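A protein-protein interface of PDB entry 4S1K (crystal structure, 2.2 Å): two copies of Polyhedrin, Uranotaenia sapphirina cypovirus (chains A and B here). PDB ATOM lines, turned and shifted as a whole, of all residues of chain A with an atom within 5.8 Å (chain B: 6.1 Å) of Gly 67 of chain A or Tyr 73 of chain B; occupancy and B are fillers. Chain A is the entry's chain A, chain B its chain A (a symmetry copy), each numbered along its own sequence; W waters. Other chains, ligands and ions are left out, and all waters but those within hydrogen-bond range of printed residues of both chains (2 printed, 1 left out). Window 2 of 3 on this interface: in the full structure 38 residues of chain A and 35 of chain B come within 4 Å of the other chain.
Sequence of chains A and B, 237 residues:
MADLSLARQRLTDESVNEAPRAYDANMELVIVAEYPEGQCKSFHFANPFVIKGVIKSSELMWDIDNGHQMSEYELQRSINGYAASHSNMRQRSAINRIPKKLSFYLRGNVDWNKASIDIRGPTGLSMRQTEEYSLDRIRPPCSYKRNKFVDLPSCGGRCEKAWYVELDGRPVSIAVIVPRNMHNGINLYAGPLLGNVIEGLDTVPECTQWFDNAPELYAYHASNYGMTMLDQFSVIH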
ATOM      1  N   ILE A  64     -25.710   1.734  -6.300  1.00  0.00           N
ATOM      2  CA  ILE A  64     -25.683   1.339  -4.897  1.00  0.00           C
ATOM      3  C   ILE A  64     -25.798  -0.158  -4.815  1.00  0.00           C
ATOM      4  O   ILE A  64     -26.508  -0.783  -5.592  1.00  0.00           O
ATOM      5  CB  ILE A  64     -26.840   1.951  -4.117  1.00  0.00           C
ATOM      6  CG1 ILE A  64     -26.924   3.469  -4.395  1.00  0.00           C
ATOM      7  CG2 ILE A  64     -26.698   1.616  -2.650  1.00  0.00           C
ATOM      8  CD1 ILE A  64     -25.634   4.207  -4.164  1.00  0.00           C
ATOM      9  N   ASP A  65     -25.096  -0.729  -3.858  1.00  0.00           N
ATOM     10  CA  ASP A  65     -24.959  -2.169  -3.750  1.00  0.00           C
ATOM     11  C   ASP A  65     -24.775  -2.440  -2.274  1.00  0.00           C
ATOM     12  O   ASP A  65     -23.748  -2.057  -1.723  1.00  0.00           O
ATOM     13  CB  ASP A  65     -23.724  -2.590  -4.558  1.00  0.00           C
ATOM     14  CG  ASP A  65     -23.279  -4.016  -4.280  1.00  0.00           C
ATOM     15  OD1 ASP A  65     -24.131  -4.894  -4.047  1.00  0.00           O
ATOM     16  OD2 ASP A  65     -22.056  -4.246  -4.317  1.00  0.00           O
ATOM     17  N   ASN A  66     -25.788  -3.010  -1.620  1.00  0.00           N
ATOM     18  CA  ASN A  66     -25.742  -3.261  -0.173  1.00  0.00           C
ATOM     19  C   ASN A  66     -25.252  -2.071   0.678  1.00  0.00           C
ATOM     20  O   ASN A  66     -24.480  -2.248   1.626  1.00  0.00           O
ATOM     21  CB  ASN A  66     -24.906  -4.533   0.108  1.00  0.00           C
ATOM     22  CG  ASN A  66     -25.699  -5.820  -0.166  1.00  0.00           C
ATOM     23  OD1 ASN A  66     -26.852  -5.951   0.270  1.00  0.00           O
ATOM     24  ND2 ASN A  66     -25.099  -6.760  -0.906  1.00  0.00           N
ATOM     25  N   GLY A  67     -25.689  -0.865   0.311  1.00  0.00           N
ATOM     26  CA  GLY A  67     -25.379   0.354   1.043  1.00  0.00           C
ATOM     27  C   GLY A  67     -24.058   1.009   0.701  1.00  0.00           C
ATOM     28  O   GLY A  67     -23.654   2.012   1.330  1.00  0.00           O
ATOM     29  N   HIS A  68     -23.388   0.453  -0.306  1.00  0.00           N
ATOM     30  CA  HIS A  68     -22.082   0.913  -0.740  1.00  0.00           C
ATOM     31  C   HIS A  68     -22.212   1.400  -2.203  1.00  0.00           C
ATOM     32  O   HIS A  68     -22.965   0.840  -2.992  1.00  0.00           O
ATOM     33  CB  HIS A  68     -21.056  -0.222  -0.593  1.00  0.00           C
ATOM     34  CG  HIS A  68     -21.144  -0.980   0.719  1.00  0.00           C
ATOM     35  ND1 HIS A  68     -21.383  -0.367   1.937  1.00  0.00           N
ATOM     36  CD2 HIS A  68     -20.993  -2.303   1.000  1.00  0.00           C
ATOM     37  CE1 HIS A  68     -21.396  -1.275   2.899  1.00  0.00           C
ATOM     38  NE2 HIS A  68     -21.154  -2.457   2.359  1.00  0.00           N
ATOM     39  N   GLN A  69     -21.491   2.457  -2.550  1.00  0.00           N
ATOM     40  CA  GLN A  69     -21.500   3.017  -3.905  1.00  0.00           C
ATOM     41  C   GLN A  69     -20.465   2.317  -4.781  1.00  0.00           C
ATOM     42  O   GLN A  69     -19.290   2.280  -4.435  1.00  0.00           O
ATOM     43  CB  GLN A  69     -21.192   4.516  -3.891  1.00  0.00           C
ATOM     44  CG  GLN A  69     -21.494   5.225  -5.211  1.00  0.00           C
ATOM     45  CD  GLN A  69     -21.325   6.742  -5.165  1.00  0.00           C
ATOM     46  OE1 GLN A  69     -21.047   7.338  -4.124  1.00  0.00           O
ATOM     47  NE2 GLN A  69     -21.511   7.378  -6.321  1.00  0.00           N
ATOM     48  N   TRP A 210     -30.097  10.057  -4.333  1.00  0.00           N
ATOM     49  CA  TRP A 210     -30.509   8.670  -4.469  1.00  0.00           C
ATOM     50  C   TRP A 210     -31.754   8.443  -3.598  1.00  0.00           C
ATOM     51  O   TRP A 210     -31.775   8.804  -2.424  1.00  0.00           O
ATOM     52  CB  TRP A 210     -29.411   7.711  -4.017  1.00  0.00           C
ATOM     53  CG  TRP A 210     -28.184   7.659  -4.875  1.00  0.00           C
ATOM     54  CD1 TRP A 210     -27.872   6.714  -5.809  1.00  0.00           C
ATOM     55  CD2 TRP A 210     -27.071   8.572  -4.842  1.00  0.00           C
ATOM     56  NE1 TRP A 210     -26.633   6.980  -6.359  1.00  0.00           N
ATOM     57  CE2 TRP A 210     -26.116   8.106  -5.781  1.00  0.00           C
ATOM     58  CE3 TRP A 210     -26.795   9.742  -4.114  1.00  0.00           C
ATOM     59  CZ2 TRP A 210     -24.910   8.775  -6.025  1.00  0.00           C
ATOM     60  CZ3 TRP A 210     -25.603  10.410  -4.361  1.00  0.00           C
ATOM     61  CH2 TRP A 210     -24.661   9.914  -5.309  1.00  0.00           C
ATOM     62  N   SER B  71     -18.007   7.447   0.156  1.00  0.00           N
ATOM     63  CA  SER B  71     -18.602   7.676  -1.153  1.00  0.00           C
ATOM     64  C   SER B  71     -19.421   8.931  -1.110  1.00  0.00           C
ATOM     65  O   SER B  71     -19.916   9.323  -0.047  1.00  0.00           O
ATOM     66  CB  SER B  71     -19.494   6.484  -1.533  1.00  0.00           C
ATOM     67  OG  SER B  71     -20.520   6.250  -0.569  1.00  0.00           O
ATOM     68  N   GLU B  72     -19.591   9.562  -2.266  1.00  0.00           N
ATOM     69  CA  GLU B  72     -20.560  10.654  -2.390  1.00  0.00           C
ATOM     70  C   GLU B  72     -21.957  10.241  -1.905  1.00  0.00           C
ATOM     71  O   GLU B  72     -22.648  10.990  -1.255  1.00  0.00           O
ATOM     72  CB  GLU B  72     -20.640  11.161  -3.824  1.00  0.00           C
ATOM     73  CG  GLU B  72     -21.581  12.345  -3.984  1.00  0.00           C
ATOM     74  CD  GLU B  72     -21.755  12.817  -5.420  1.00  0.00           C
ATOM     75  OE1 GLU B  72     -21.000  12.335  -6.296  1.00  0.00           O
ATOM     76  OE2 GLU B  72     -22.650  13.678  -5.672  1.00  0.00           O
ATOM     77  N   TYR B  73     -22.368   9.035  -2.228  1.00  0.00           N
ATOM     78  CA  TYR B  73     -23.641   8.515  -1.754  1.00  0.00           C
ATOM     79  C   TYR B  73     -23.774   8.546  -0.221  1.00  0.00           C
ATOM     80  O   TYR B  73     -24.785   9.020   0.295  1.00  0.00           O
ATOM     81  CB  TYR B  73     -23.876   7.107  -2.310  1.00  0.00           C
ATOM     82  CG  TYR B  73     -24.961   6.379  -1.558  1.00  0.00           C
ATOM     83  CD1 TYR B  73     -26.304   6.579  -1.865  1.00  0.00           C
ATOM     84  CD2 TYR B  73     -24.652   5.494  -0.536  1.00  0.00           C
ATOM     85  CE1 TYR B  73     -27.305   5.901  -1.186  1.00  0.00           C
ATOM     86  CE2 TYR B  73     -25.629   4.807   0.125  1.00  0.00           C
ATOM     87  CZ  TYR B  73     -26.958   5.018  -0.191  1.00  0.00           C
ATOM     88  OH  TYR B  73     -27.937   4.361   0.524  1.00  0.00           O
ATOM     89  N   GLU B  74     -22.776   8.054   0.517  1.00  0.00           N
ATOM     90  CA  GLU B  74     -22.864   8.069   2.004  1.00  0.00           C
ATOM     91  C   GLU B  74     -22.899   9.495   2.515  1.00  0.00           C
ATOM     92  O   GLU B  74     -23.641   9.841   3.435  1.00  0.00           O
ATOM     93  CB  GLU B  74     -21.650   7.451   2.677  1.00  0.00           C
ATOM     94  CG  GLU B  74     -21.382   5.986   2.440  1.00  0.00           C
ATOM     95  CD  GLU B  74     -19.978   5.630   2.916  1.00  0.00           C
ATOM     96  OE1 GLU B  74     -19.145   5.145   2.105  1.00  0.00           O
ATOM     97  OE2 GLU B  74     -19.715   5.885   4.124  1.00  0.00           O
ATOM     98  N   LEU B  75     -22.045  10.327   1.944  1.00  0.00           N
ATOM     99  CA  LEU B  75     -21.997  11.699   2.407  1.00  0.00           C
ATOM    100  C   LEU B  75     -23.315  12.421   2.072  1.00  0.00           C
ATOM    101  O   LEU B  75     -23.874  13.115   2.919  1.00  0.00           O
ATOM    102  CB  LEU B  75     -20.820  12.423   1.799  1.00  0.00           C
ATOM    103  CG  LEU B  75     -19.460  11.812   2.110  1.00  0.00           C
ATOM    104  CD1 LEU B  75     -18.454  12.286   1.067  1.00  0.00           C
ATOM    105  CD2 LEU B  75     -19.026  12.165   3.518  1.00  0.00           C
ATOM    106  N   GLN B  76     -23.831  12.218   0.859  1.00  0.00           N
ATOM    107  CA  GLN B  76     -25.048  12.884   0.484  1.00  0.00           C
ATOM    108  C   GLN B  76     -26.184  12.342   1.335  1.00  0.00           C
ATOM    109  O   GLN B  76     -27.071  13.076   1.654  1.00  0.00           O
ATOM    110  CB  GLN B  76     -25.377  12.732  -0.996  1.00  0.00           C
ATOM    111  CG  GLN B  76     -26.570  13.579  -1.449  1.00  0.00           C
ATOM    112  CD  GLN B  76     -26.354  15.092  -1.257  1.00  0.00           C
ATOM    113  OE1 GLN B  76     -25.274  15.611  -1.523  1.00  0.00           O
ATOM    114  NE2 GLN B  76     -27.393  15.801  -0.810  1.00  0.00           N
ATOM    115  N   ARG B  77     -26.145  11.085   1.750  1.00  0.00           N
ATOM    116  CA  ARG B  77     -27.206  10.573   2.600  1.00  0.00           C
ATOM    117  C   ARG B  77     -27.302  11.347   3.934  1.00  0.00           C
ATOM    118  O   ARG B  77     -28.397  11.691   4.377  1.00  0.00           O
ATOM    119  CB  ARG B  77     -27.009   9.091   2.845  1.00  0.00           C
ATOM    120  CG  ARG B  77     -28.080   8.506   3.753  1.00  0.00           C
ATOM    121  CD  ARG B  77     -28.013   7.007   3.710  1.00  0.00           C
ATOM    122  NE  ARG B  77     -26.733   6.573   4.241  1.00  0.00           N
ATOM    123  CZ  ARG B  77     -26.256   5.336   4.118  1.00  0.00           C
ATOM    124  NH1 ARG B  77     -26.966   4.393   3.473  1.00  0.00           N
ATOM    125  NH2 ARG B  77     -25.064   5.046   4.639  1.00  0.00           N
ATOM    126  N   SER B  78     -26.150  11.619   4.552  1.00  0.00           N
ATOM    127  CA  SER B  78     -26.077  12.424   5.772  1.00  0.00           C
ATOM    128  C   SER B  78     -26.549  13.851   5.565  1.00  0.00           C
ATOM    129  O   SER B  78     -27.255  14.405   6.402  1.00  0.00           O
ATOM    130  CB  SER B  78     -24.646  12.471   6.320  1.00  0.00           C
ATOM    131  OG  SER B  78     -24.254  11.204   6.828  1.00  0.00           O
HETATM  132  O   HOH W   1     -18.054   8.754  -4.423  1.00  0.00           O
HETATM  133  O   HOH W   2     -20.542   3.851   0.116  1.00  0.00           O
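The backbone NH of Glu 72 of chain B is in hydrogen-bond range of the side-chain amide oxygen of Gln 69 of chain A, at 3.2 Å.
The side-chain amide oxygen of Gln 69 of chain A lies within hydrogen-bond range of the backbone NH of Tyr 73 of chain B (2.9 Å).
The backbone NH (N) of Glu 74 of chain B is in hydrogen-bond range of the side-chain hydroxyl (OG) of Ser 71 of chain B, 3.1 Å away.
NH1 of Arg 77 of chain B sits at hydrogen-bond distance from OH of Tyr 73 of chain B (3.1 Å).
Tyr 73 of chain B touches Ile 64 of chain A (CD1 to CD1, 3.4 Å).
Gly 67 of chain A touches Tyr 73 of chain B.
Ser 71 of chain B touches Gln 69 of chain A.
Trp 210 of chain A touches Tyr 73 of chain B (CD2 to CD1, 3.7 Å).
Gly 67 of chain A touches just one residue of chain B: Tyr 73 (3.6 Å).
Tyr 73 of chain B touches four residues of chain A.
Of the printed residues of chain A, Ser 71 of chain B touches Gln 69.
Of the printed residues of chain B, Trp 210 of chain A touches Tyr 73 (3.7 Å).
Gln 76 of chain B touches none of the printed residues of chain A.
Ser 78 of chain B touches none of the printed residues of chain A.
The nearest residue of chain A that does not touch Tyr 73 of chain B is His 68 of chain A (4.9 Å).
Of the 8 printed residues of chain B, 3 touch a printed residue of chain A.
Hydrophobic or aromatic side chains of chain A within 4 Å of the printed part of chain B: Ile 64 and Trp 210.
Among the printed residues, 6 pairs touch across the chains.
No position is printed for both chains.
Water W2 lies within hydrogen-bond range of OG of Ser 71 of chain B (2.5 Å), OE1 of Glu 74 of chain B (2.8 Å) and N of Gln 69 of chain A (3.2 Å).
Water W1 bridges N of Glu 72 of chain B (2.8 Å) and OE1 of Gln 69 of chain A (3.3 Å).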
